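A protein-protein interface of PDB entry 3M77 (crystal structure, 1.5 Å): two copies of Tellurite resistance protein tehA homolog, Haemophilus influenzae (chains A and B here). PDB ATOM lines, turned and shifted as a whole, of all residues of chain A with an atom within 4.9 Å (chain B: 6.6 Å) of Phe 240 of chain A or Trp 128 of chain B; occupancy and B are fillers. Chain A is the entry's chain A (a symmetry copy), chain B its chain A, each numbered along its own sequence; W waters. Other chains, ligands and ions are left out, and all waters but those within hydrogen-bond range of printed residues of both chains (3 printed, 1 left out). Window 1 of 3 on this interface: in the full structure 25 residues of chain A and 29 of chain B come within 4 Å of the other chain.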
ATOM      1  N   LEU A 185     -18.400 -10.703 -23.735  1.00  0.00           N
ATOM      2  CA  LEU A 185     -17.904 -10.937 -22.382  1.00  0.00           C
ATOM      3  C   LEU A 185     -19.045 -11.309 -21.425  1.00  0.00           C
ATOM      4  O   LEU A 185     -18.871 -12.115 -20.497  1.00  0.00           O
ATOM      5  CB  LEU A 185     -17.077  -9.791 -21.827  1.00  0.00           C
ATOM      6  CG  LEU A 185     -15.839  -9.433 -22.659  1.00  0.00           C
ATOM      7  CD1 LEU A 185     -14.944  -8.396 -21.960  1.00  0.00           C
ATOM      8  CD2 LEU A 185     -15.033 -10.616 -23.073  1.00  0.00           C
ATOM      9  N   LEU A 188     -19.723 -14.942 -22.032  1.00  0.00           N
ATOM     10  CA  LEU A 188     -18.712 -15.802 -21.429  1.00  0.00           C
ATOM     11  C   LEU A 188     -18.907 -15.889 -19.908  1.00  0.00           C
ATOM     12  O   LEU A 188     -18.721 -16.954 -19.305  1.00  0.00           O
ATOM     13  CB  LEU A 188     -17.298 -15.298 -21.734  1.00  0.00           C
ATOM     14  CG  LEU A 188     -16.886 -15.355 -23.191  1.00  0.00           C
ATOM     15  CD1 LEU A 188     -15.509 -14.776 -23.326  1.00  0.00           C
ATOM     16  CD2 LEU A 188     -16.903 -16.779 -23.717  1.00  0.00           C
ATOM     17  N   ARG A 189     -19.244 -14.754 -19.284  1.00  0.00           N
ATOM     18  CA  ARG A 189     -19.493 -14.754 -17.851  1.00  0.00           C
ATOM     19  C   ARG A 189     -20.609 -15.735 -17.455  1.00  0.00           C
ATOM     20  O   ARG A 189     -20.534 -16.419 -16.416  1.00  0.00           O
ATOM     21  CB  ARG A 189     -19.835 -13.348 -17.341  1.00  0.00           C
ATOM     22  CG  ARG A 189     -18.650 -12.423 -17.139  1.00  0.00           C
ATOM     23  CD  ARG A 189     -19.072 -11.171 -16.397  1.00  0.00           C
ATOM     24  NE  ARG A 189     -19.857 -10.236 -17.227  1.00  0.00           N
ATOM     25  CZ  ARG A 189     -19.328  -9.286 -17.984  1.00  0.00           C
ATOM     26  NH1 ARG A 189     -18.015  -9.115 -18.015  1.00  0.00           N
ATOM     27  NH2 ARG A 189     -20.103  -8.480 -18.688  1.00  0.00           N
ATOM     28  N   MET A 201     -10.681 -18.778 -27.263  1.00  0.00           N
ATOM     29  CA  MET A 201     -10.449 -17.687 -26.327  1.00  0.00           C
ATOM     30  C   MET A 201      -9.203 -16.898 -26.705  1.00  0.00           C
ATOM     31  O   MET A 201      -9.060 -15.713 -26.342  1.00  0.00           O
ATOM     32  CB  MET A 201     -10.303 -18.194 -24.894  1.00  0.00           C
ATOM     33  CG  MET A 201     -11.591 -18.702 -24.311  1.00  0.00           C
ATOM     34  SD  MET A 201     -12.861 -17.460 -24.104  1.00  0.00           S
ATOM     35  CE  MET A 201     -12.072 -16.371 -22.904  1.00  0.00           C
ATOM     36  N   VAL A 204      -9.700 -13.503 -28.195  1.00  0.00           N
ATOM     37  CA  VAL A 204     -10.000 -12.379 -27.311  1.00  0.00           C
ATOM     38  C   VAL A 204      -8.751 -11.516 -27.105  1.00  0.00           C
ATOM     39  O   VAL A 204      -8.872 -10.327 -26.775  1.00  0.00           O
ATOM     40  CB  VAL A 204     -10.624 -12.886 -25.955  1.00  0.00           C
ATOM     41  CG1 VAL A 204     -10.875 -11.731 -25.032  1.00  0.00           C
ATOM     42  CG2 VAL A 204     -11.951 -13.654 -26.249  1.00  0.00           C
ATOM     43  N   LEU A 236      -4.350  -5.751 -20.143  1.00  0.00           N
ATOM     44  CA  LEU A 236      -5.371  -6.264 -19.228  1.00  0.00           C
ATOM     45  C   LEU A 236      -5.896  -7.620 -19.701  1.00  0.00           C
ATOM     46  O   LEU A 236      -5.961  -8.585 -18.945  1.00  0.00           O
ATOM     47  CB  LEU A 236      -6.521  -5.255 -19.113  1.00  0.00           C
ATOM     48  CG  LEU A 236      -7.592  -5.654 -18.099  1.00  0.00           C
ATOM     49  CD1 LEU A 236      -7.130  -5.409 -16.703  1.00  0.00           C
ATOM     50  CD2 LEU A 236      -8.890  -4.856 -18.343  1.00  0.00           C
ATOM     51  N   GLN A 237      -6.299  -7.683 -20.965  1.00  0.00           N
ATOM     52  CA  GLN A 237      -6.808  -8.919 -21.557  1.00  0.00           C
ATOM     53  C   GLN A 237      -5.775 -10.035 -21.580  1.00  0.00           C
ATOM     54  O   GLN A 237      -6.089 -11.179 -21.291  1.00  0.00           O
ATOM     55  CB  GLN A 237      -7.317  -8.661 -22.971  1.00  0.00           C
ATOM     56  CG  GLN A 237      -8.473  -7.639 -23.104  1.00  0.00           C
ATOM     57  CD  GLN A 237      -9.755  -8.050 -22.381  1.00  0.00           C
ATOM     58  OE1 GLN A 237      -9.809  -8.085 -21.120  1.00  0.00           O
ATOM     59  NE2 GLN A 237     -10.797  -8.363 -23.170  1.00  0.00           N
ATOM     60  N   LEU A 238      -4.530  -9.678 -21.855  1.00  0.00           N
ATOM     61  CA  LEU A 238      -3.432 -10.659 -21.773  1.00  0.00           C
ATOM     62  C   LEU A 238      -3.338 -11.268 -20.383  1.00  0.00           C
ATOM     63  O   LEU A 238      -3.274 -12.470 -20.222  1.00  0.00           O
ATOM     64  CB  LEU A 238      -2.120 -10.001 -22.139  1.00  0.00           C
ATOM     65  CG  LEU A 238      -0.911 -10.911 -21.954  1.00  0.00           C
ATOM     66  CD1 LEU A 238      -0.951 -12.050 -22.923  1.00  0.00           C
ATOM     67  CD2 LEU A 238       0.361 -10.105 -22.142  1.00  0.00           C
ATOM     68  N   PHE A 239      -3.373 -10.418 -19.371  1.00  0.00           N
ATOM     69  CA  PHE A 239      -3.233 -10.917 -18.006  1.00  0.00           C
ATOM     70  C   PHE A 239      -4.410 -11.837 -17.672  1.00  0.00           C
ATOM     71  O   PHE A 239      -4.236 -12.876 -17.063  1.00  0.00           O
ATOM     72  CB  PHE A 239      -3.178  -9.790 -16.985  1.00  0.00           C
ATOM     73  CG  PHE A 239      -1.977  -8.889 -17.117  1.00  0.00           C
ATOM     74  CD1 PHE A 239      -0.827  -9.284 -17.769  1.00  0.00           C
ATOM     75  CD2 PHE A 239      -2.058  -7.610 -16.647  1.00  0.00           C
ATOM     76  CE1 PHE A 239       0.259  -8.416 -17.898  1.00  0.00           C
ATOM     77  CE2 PHE A 239      -0.969  -6.749 -16.768  1.00  0.00           C
ATOM     78  CZ  PHE A 239       0.182  -7.168 -17.375  1.00  0.00           C
ATOM     79  N   PHE A 240      -5.609 -11.442 -18.078  1.00  0.00           N
ATOM     80  CA  PHE A 240      -6.777 -12.278 -17.849  1.00  0.00           C
ATOM     81  C   PHE A 240      -6.627 -13.648 -18.544  1.00  0.00           C
ATOM     82  O   PHE A 240      -6.921 -14.691 -17.947  1.00  0.00           O
ATOM     83  CB  PHE A 240      -8.065 -11.603 -18.360  1.00  0.00           C
ATOM     84  CG  PHE A 240      -8.550 -10.443 -17.524  1.00  0.00           C
ATOM     85  CD1 PHE A 240      -7.861  -9.956 -16.425  1.00  0.00           C
ATOM     86  CD2 PHE A 240      -9.730  -9.841 -17.860  1.00  0.00           C
ATOM     87  CE1 PHE A 240      -8.352  -8.885 -15.698  1.00  0.00           C
ATOM     88  CE2 PHE A 240     -10.199  -8.748 -17.140  1.00  0.00           C
ATOM     89  CZ  PHE A 240      -9.542  -8.294 -16.075  1.00  0.00           C
ATOM     90  N   LEU A 241      -6.148 -13.647 -19.786  1.00  0.00           N
ATOM     91  CA  LEU A 241      -6.032 -14.881 -20.543  1.00  0.00           C
ATOM     92  C   LEU A 241      -4.913 -15.760 -20.009  1.00  0.00           C
ATOM     93  O   LEU A 241      -5.012 -16.984 -20.008  1.00  0.00           O
ATOM     94  CB  LEU A 241      -5.884 -14.577 -22.034  1.00  0.00           C
ATOM     95  CG  LEU A 241      -7.141 -14.016 -22.674  1.00  0.00           C
ATOM     96  CD1 LEU A 241      -6.775 -13.415 -24.022  1.00  0.00           C
ATOM     97  CD2 LEU A 241      -8.196 -15.116 -22.852  1.00  0.00           C
ATOM     98  N   LEU A 242      -3.854 -15.134 -19.525  1.00  0.00           N
ATOM     99  CA  LEU A 242      -2.776 -15.892 -18.864  1.00  0.00           C
ATOM    100  C   LEU A 242      -3.334 -16.637 -17.630  1.00  0.00           C
ATOM    101  O   LEU A 242      -3.099 -17.854 -17.458  1.00  0.00           O
ATOM    102  CB  LEU A 242      -1.630 -14.957 -18.474  1.00  0.00           C
ATOM    103  CG  LEU A 242      -0.703 -14.552 -19.606  1.00  0.00           C
ATOM    104  CD1 LEU A 242       0.182 -13.435 -19.174  1.00  0.00           C
ATOM    105  CD2 LEU A 242       0.129 -15.745 -20.063  1.00  0.00           C
ATOM    106  N   ARG A 243      -4.139 -15.945 -16.817  1.00  0.00           N
ATOM    107  CA  ARG A 243      -4.726 -16.582 -15.642  1.00  0.00           C
ATOM    108  C   ARG A 243      -5.694 -17.702 -16.033  1.00  0.00           C
ATOM    109  O   ARG A 243      -5.748 -18.736 -15.363  1.00  0.00           O
ATOM    110  CB  ARG A 243      -5.427 -15.574 -14.745  1.00  0.00           C
ATOM    111  CG  ARG A 243      -5.944 -16.177 -13.449  1.00  0.00           C
ATOM    112  CD  ARG A 243      -4.823 -16.802 -12.606  1.00  0.00           C
ATOM    113  NE  ARG A 243      -5.369 -17.506 -11.448  1.00  0.00           N
ATOM    114  CZ  ARG A 243      -4.643 -18.155 -10.548  1.00  0.00           C
ATOM    115  NH1 ARG A 243      -3.328 -18.214 -10.668  1.00  0.00           N
ATOM    116  NH2 ARG A 243      -5.238 -18.747  -9.528  1.00  0.00           N
ATOM    117  N   LEU A 244      -6.393 -17.523 -17.133  1.00  0.00           N
ATOM    118  CA  LEU A 244      -7.353 -18.483 -17.617  1.00  0.00           C
ATOM    119  C   LEU A 244      -6.717 -19.621 -18.390  1.00  0.00           C
ATOM    120  O   LEU A 244      -7.409 -20.583 -18.740  1.00  0.00           O
ATOM    121  CB  LEU A 244      -8.369 -17.790 -18.502  1.00  0.00           C
ATOM    122  CG  LEU A 244      -9.395 -16.907 -17.792  1.00  0.00           C
ATOM    123  CD1 LEU A 244     -10.095 -16.018 -18.746  1.00  0.00           C
ATOM    124  CD2 LEU A 244     -10.381 -17.802 -17.049  1.00  0.00           C
ATOM    125  N   TRP A 247      -7.458 -23.391 -17.592  1.00  0.00           N
ATOM    126  CA  TRP A 247      -8.846 -23.693 -17.963  1.00  0.00           C
ATOM    127  C   TRP A 247      -8.991 -23.790 -19.475  1.00  0.00           C
ATOM    128  O   TRP A 247      -9.665 -24.697 -20.008  1.00  0.00           O
ATOM    129  CB  TRP A 247      -9.777 -22.626 -17.383  1.00  0.00           C
ATOM    130  CG  TRP A 247     -11.210 -22.656 -17.814  1.00  0.00           C
ATOM    131  CD1 TRP A 247     -12.248 -23.439 -17.295  1.00  0.00           C
ATOM    132  CD2 TRP A 247     -11.797 -21.862 -18.834  1.00  0.00           C
ATOM    133  NE1 TRP A 247     -13.415 -23.145 -17.949  1.00  0.00           N
ATOM    134  CE2 TRP A 247     -13.170 -22.187 -18.895  1.00  0.00           C
ATOM    135  CE3 TRP A 247     -11.301 -20.863 -19.693  1.00  0.00           C
ATOM    136  CZ2 TRP A 247     -14.037 -21.592 -19.807  1.00  0.00           C
ATOM    137  CZ3 TRP A 247     -12.164 -20.281 -20.600  1.00  0.00           C
ATOM    138  CH2 TRP A 247     -13.516 -20.630 -20.645  1.00  0.00           C
ATOM    139  N   LEU B 117      -4.585  -4.911  -9.518  1.00  0.00           N
ATOM    140  CA  LEU B 117      -4.350  -5.616 -10.747  1.00  0.00           C
ATOM    141  C   LEU B 117      -4.356  -7.122 -10.471  1.00  0.00           C
ATOM    142  O   LEU B 117      -4.911  -7.891 -11.256  1.00  0.00           O
ATOM    143  CB  LEU B 117      -3.050  -5.162 -11.397  1.00  0.00           C
ATOM    144  CG  LEU B 117      -2.666  -5.755 -12.738  1.00  0.00           C
ATOM    145  CD1 LEU B 117      -3.786  -5.505 -13.756  1.00  0.00           C
ATOM    146  CD2 LEU B 117      -1.315  -5.100 -13.160  1.00  0.00           C
ATOM    147  N   SER B 120      -8.155  -8.164  -9.897  1.00  0.00           N
ATOM    148  CA  SER B 120      -8.956  -8.320 -11.103  1.00  0.00           C
ATOM    149  C   SER B 120      -8.457  -9.477 -11.931  1.00  0.00           C
ATOM    150  O   SER B 120      -9.248 -10.243 -12.457  1.00  0.00           O
ATOM    151  CB  SER B 120      -8.933  -7.038 -11.935  1.00  0.00           C
ATOM    152  OG  SER B 120      -7.642  -6.813 -12.461  1.00  0.00           O
ATOM    153  N   THR B 121      -7.131  -9.615 -12.050  1.00  0.00           N
ATOM    154  CA  THR B 121      -6.584 -10.704 -12.839  1.00  0.00           C
ATOM    155  C   THR B 121      -7.028 -12.059 -12.293  1.00  0.00           C
ATOM    156  O   THR B 121      -7.337 -12.998 -13.058  1.00  0.00           O
ATOM    157  CB  THR B 121      -5.044 -10.622 -12.885  1.00  0.00           C
ATOM    158  OG1 THR B 121      -4.692  -9.444 -13.616  1.00  0.00           O
ATOM    159  CG2 THR B 121      -4.496 -11.825 -13.578  1.00  0.00           C
ATOM    160  N   LEU B 122      -7.102 -12.172 -10.971  1.00  0.00           N
ATOM    161  CA  LEU B 122      -7.584 -13.421 -10.391  1.00  0.00           C
ATOM    162  C   LEU B 122      -9.095 -13.602 -10.528  1.00  0.00           C
ATOM    163  O   LEU B 122      -9.561 -14.669 -10.939  1.00  0.00           O
ATOM    164  CB  LEU B 122      -7.186 -13.530  -8.952  1.00  0.00           C
ATOM    165  CG  LEU B 122      -5.694 -13.689  -8.725  1.00  0.00           C
ATOM    166  CD1 LEU B 122      -5.315 -13.441  -7.225  1.00  0.00           C
ATOM    167  CD2 LEU B 122      -5.277 -15.034  -9.211  1.00  0.00           C
ATOM    168  N   ARG B 123      -9.870 -12.592 -10.150  1.00  0.00           N
ATOM    169  CA  ARG B 123     -11.302 -12.765  -9.993  1.00  0.00           C
ATOM    170  C   ARG B 123     -12.149 -12.363 -11.176  1.00  0.00           C
ATOM    171  O   ARG B 123     -13.118 -13.051 -11.503  1.00  0.00           O
ATOM    172  CB  ARG B 123     -11.765 -12.004  -8.754  1.00  0.00           C
ATOM    173  CG  ARG B 123     -11.439 -12.759  -7.543  1.00  0.00           C
ATOM    174  CD  ARG B 123     -12.229 -14.091  -7.470  1.00  0.00           C
ATOM    175  NE  ARG B 123     -13.637 -13.811  -7.291  1.00  0.00           N
ATOM    176  CZ  ARG B 123     -14.611 -14.203  -8.097  1.00  0.00           C
ATOM    177  NH1 ARG B 123     -14.367 -14.958  -9.152  1.00  0.00           N
ATOM    178  NH2 ARG B 123     -15.846 -13.844  -7.830  1.00  0.00           N
ATOM    179  N   VAL B 124     -11.831 -11.237 -11.812  1.00  0.00           N
ATOM    180  CA  VAL B 124     -12.629 -10.745 -12.932  1.00  0.00           C
ATOM    181  C   VAL B 124     -12.509 -11.735 -14.112  1.00  0.00           C
ATOM    182  O   VAL B 124     -13.524 -12.091 -14.731  1.00  0.00           O
ATOM    183  CB  VAL B 124     -12.300  -9.317 -13.337  1.00  0.00           C
ATOM    184  CG1 VAL B 124     -13.057  -8.913 -14.655  1.00  0.00           C
ATOM    185  CG2 VAL B 124     -12.602  -8.365 -12.181  1.00  0.00           C
ATOM    186  N   SER B 125     -11.297 -12.206 -14.376  1.00  0.00           N
ATOM    187  CA  SER B 125     -11.080 -13.162 -15.439  1.00  0.00           C
ATOM    188  C   SER B 125     -11.783 -14.490 -15.161  1.00  0.00           C
ATOM    189  O   SER B 125     -12.309 -15.115 -16.073  1.00  0.00           O
ATOM    190  CB  SER B 125      -9.598 -13.405 -15.633  1.00  0.00           C
ATOM    191  OG  SER B 125      -9.050 -14.122 -14.539  1.00  0.00           O
ATOM    192  N   GLU B 126     -11.784 -14.908 -13.899  1.00  0.00           N
ATOM    193  CA  GLU B 126     -12.378 -16.163 -13.532  1.00  0.00           C
ATOM    194  C   GLU B 126     -13.845 -16.242 -13.927  1.00  0.00           C
ATOM    195  O   GLU B 126     -14.352 -17.307 -14.240  1.00  0.00           O
ATOM    196  CB  GLU B 126     -12.224 -16.366 -12.021  1.00  0.00           C
ATOM    197  CG  GLU B 126     -12.651 -17.725 -11.580  1.00  0.00           C
ATOM    198  CD  GLU B 126     -12.399 -17.973 -10.089  1.00  0.00           C
ATOM    199  OE1 GLU B 126     -12.209 -16.998  -9.315  1.00  0.00           O
ATOM    200  OE2 GLU B 126     -12.390 -19.163  -9.703  1.00  0.00           O
ATOM    201  N   LEU B 127     -14.517 -15.100 -13.912  1.00  0.00           N
ATOM    202  CA  LEU B 127     -15.933 -15.026 -14.303  1.00  0.00           C
ATOM    203  C   LEU B 127     -16.145 -15.593 -15.722  1.00  0.00           C
ATOM    204  O   LEU B 127     -17.209 -16.150 -16.014  1.00  0.00           O
ATOM    205  CB  LEU B 127     -16.503 -13.611 -14.170  1.00  0.00           C
ATOM    206  CG  LEU B 127     -16.445 -12.926 -12.818  1.00  0.00           C
ATOM    207  CD1 LEU B 127     -16.905 -11.507 -12.893  1.00  0.00           C
ATOM    208  CD2 LEU B 127     -17.311 -13.674 -11.807  1.00  0.00           C
ATOM    209  N   TRP B 128     -15.132 -15.434 -16.592  1.00  0.00           N
ATOM    210  CA  TRP B 128     -15.252 -15.880 -17.969  1.00  0.00           C
ATOM    211  C   TRP B 128     -15.302 -17.388 -18.149  1.00  0.00           C
ATOM    212  O   TRP B 128     -15.560 -17.867 -19.255  1.00  0.00           O
ATOM    213  CB  TRP B 128     -14.139 -15.318 -18.868  1.00  0.00           C
ATOM    214  CG  TRP B 128     -14.028 -13.847 -19.043  1.00  0.00           C
ATOM    215  CD1 TRP B 128     -14.825 -12.873 -18.570  1.00  0.00           C
ATOM    216  CD2 TRP B 128     -12.996 -13.201 -19.769  1.00  0.00           C
ATOM    217  NE1 TRP B 128     -14.349 -11.633 -18.941  1.00  0.00           N
ATOM    218  CE2 TRP B 128     -13.205 -11.816 -19.671  1.00  0.00           C
ATOM    219  CE3 TRP B 128     -11.891 -13.665 -20.465  1.00  0.00           C
ATOM    220  CZ2 TRP B 128     -12.357 -10.897 -20.254  1.00  0.00           C
ATOM    221  CZ3 TRP B 128     -11.052 -12.738 -21.047  1.00  0.00           C
ATOM    222  CH2 TRP B 128     -11.293 -11.387 -20.953  1.00  0.00           C
ATOM    223  N   GLN B 129     -15.093 -18.160 -17.066  1.00  0.00           N
ATOM    224  CA  GLN B 129     -15.277 -19.591 -17.082  1.00  0.00           C
ATOM    225  C   GLN B 129     -16.738 -19.997 -17.106  1.00  0.00           C
ATOM    226  O   GLN B 129     -17.065 -21.140 -17.412  1.00  0.00           O
ATOM    227  CB  GLN B 129     -14.601 -20.232 -15.867  1.00  0.00           C
ATOM    228  CG  GLN B 129     -13.118 -19.961 -15.822  1.00  0.00           C
ATOM    229  CD  GLN B 129     -12.442 -20.554 -14.595  1.00  0.00           C
ATOM    230  OE1 GLN B 129     -13.109 -20.988 -13.650  1.00  0.00           O
ATOM    231  NE2 GLN B 129     -11.115 -20.519 -14.581  1.00  0.00           N
ATOM    232  N   GLY B 130     -17.615 -19.069 -16.773  1.00  0.00           N
ATOM    233  CA  GLY B 130     -19.054 -19.289 -16.863  1.00  0.00           C
ATOM    234  C   GLY B 130     -19.638 -20.046 -15.688  1.00  0.00           C
ATOM    235  O   GLY B 130     -18.929 -20.649 -14.902  1.00  0.00           O
ATOM    236  N   PHE B 142     -19.830  -3.897 -10.237  1.00  0.00           N
ATOM    237  CA  PHE B 142     -18.799  -4.445 -11.128  1.00  0.00           C
ATOM    238  C   PHE B 142     -17.847  -3.379 -11.636  1.00  0.00           C
ATOM    239  O   PHE B 142     -16.682  -3.663 -11.895  1.00  0.00           O
ATOM    240  CB  PHE B 142     -19.456  -5.282 -12.243  1.00  0.00           C
ATOM    241  CG  PHE B 142     -18.496  -5.944 -13.188  1.00  0.00           C
ATOM    242  CD1 PHE B 142     -18.061  -7.226 -12.930  1.00  0.00           C
ATOM    243  CD2 PHE B 142     -18.044  -5.286 -14.350  1.00  0.00           C
ATOM    244  CE1 PHE B 142     -17.203  -7.863 -13.827  1.00  0.00           C
ATOM    245  CE2 PHE B 142     -17.136  -5.902 -15.209  1.00  0.00           C
ATOM    246  CZ  PHE B 142     -16.762  -7.215 -14.932  1.00  0.00           C
HETATM  247  O   HOH W   1     -16.062 -23.790 -17.479  1.00  0.00           O
HETATM  248  O   HOH W   2     -15.690 -10.303 -16.403  1.00  0.00           O
HETATM  249  O   HOH W   3     -14.640  -8.351 -18.080  1.00  0.00           O
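Of the 15 printed residues of chain A, 10 touch a printed residue of chain B. Of the 13 printed residues of chain B, 11 touch a printed residue of chain A. Among the printed residues, 24 pairs touch across the chains. Among the printed residues, no Asp or Glu carboxylate lies within 4 Å of a Lys or Arg side-chain nitrogen of the other chain.
Water W1 lies within hydrogen-bond range of the indole nitrogen (NE1) of Trp 247 of chain A and the backbone carbonyl oxygen (O) of Gln 129 of chain B. Water W2 lies within hydrogen-bond range of NH1 of Arg 189 of chain A, NE1 of Trp 128 of chain B and O of Val 124 of chain B. Water W3 lies within hydrogen-bond range of NE1 of Trp 128 of chain B (3.4 Å) and NH1 of Arg 189 of chain A (3.5 Å).
The backbone carbonyl oxygen of Leu 117 of chain B sits at hydrogen-bond distance from the side-chain hydroxyl of Ser 120 of chain B. The backbone carbonyl oxygen (O) of Leu 117 of chain B sits at hydrogen-bond distance from the side-chain hydroxyl (OG1) of Thr 121 of chain B, 2.8 Å away. The backbone carbonyl oxygen (O) of Ser 120 of chain B sits at hydrogen-bond distance from the backbone NH (N) of Ser 125 of chain B (3.4 Å). O of Thr 121 of chain B sits at hydrogen-bond distance from OG of Ser 125 of chain B (2.5 Å).
No position is printed for both chains. Of the 24 pairs that touch across the chains among the printed residues, none has its exchanged pair printed and touching as well.
The backbone NH (N) of Gly 130 of chain B lies close to the backbone carbonyl oxygen (O) of Leu 188 of chain A (3.5 Å). The backbone carbonyl oxygen (O) of Leu 188 of chain A lies close to the backbone carbonyl oxygen (O) of Trp 128 of chain B. O of Leu 127 of chain B sits close to O of Arg 189 of chain A.
Printed residues of chain B within 4 Å of Phe 240 of chain A: Ser 120, Thr 121, Val 124, Ser 125 and Trp 128. Leu 242 of chain A touches none of the printed residues of chain B. Of the printed residues of chain B, Trp 247 of chain A touches Trp 128 (3.7 Å) and Gln 129 (3.6 Å). Printed residues of chain A within 4 Å of Leu 117 of chain B: Phe 239. Of the printed residues of chain A, Leu 127 of chain B touches Leu 188 and Arg 189. Of the printed residues of chain A, Trp 128 of chain B touches Leu 185, Leu 188, Met 201, Gln 237, Phe 240, Leu 244 and Trp 247. Printed residues of chain A within 4 Å of Gly 130 of chain B: Leu 188 (3.4 Å) and Arg 189 (3.3 Å). The nearest printed residue of chain B that does not touch Phe 240 of chain A is Leu 117 of chain B (5.7 Å). The nearest printed residue of chain A that does not touch Trp 128 of chain B is Arg 189 of chain A (4.1 Å). The nearest printed residue of chain A that does not touch Ser 120 of chain B is Leu 236 of chain A (4.5 Å).
Among the printed residues, pairs that only touch across the chains: Leu 185 of chain A with Trp 128 of chain B (3.9 Å), Leu 188 of chain A with Leu 127 of chain B (3.7 Å), Arg 189 of chain A with Gly 130 of chain B (3.3 Å), Arg 189 of chain A with Phe 142 of chain B (3.8 Å), Met 201 of chain A with Trp 128 of chain B (3.6 Å), Gln 237 of chain A with Trp 128 of chain B (3.6 Å), Phe 239 of chain A with Leu 117 of chain B (3.97 Å), Phe 239 of chain A with Thr 121 of chain B (3.6 Å), Phe 240 of chain A with Ser 120 of chain B (3.6 Å), Phe 240 of chain A with Thr 121 of chain B (3.8 Å), Phe 240 of chain A with Val 124 of chain B (3.8 Å), Phe 240 of chain A with Ser 125 of chain B (3.6 Å), Phe 240 of chain A with Trp 128 of chain B (3.7 Å), Arg 243 of chain A with Thr 121 of chain B (3.5 Å), Arg 243 of chain A with Leu 122 of chain B (3.3 Å), Arg 243 of chain A with Ser 125 of chain B (3.9 Å), Leu 244 of chain A with Ser 125 of chain B (3.4 Å), Leu 244 of chain A with Trp 128 of chain B (3.4 Å), Leu 244 of chain A with Gln 129 of chain B (3.7 Å), Trp 247 of chain A with Trp 128 of chain B (3.7 Å) and Trp 247 of chain A with Gln 129 of chain B (3.6 Å).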
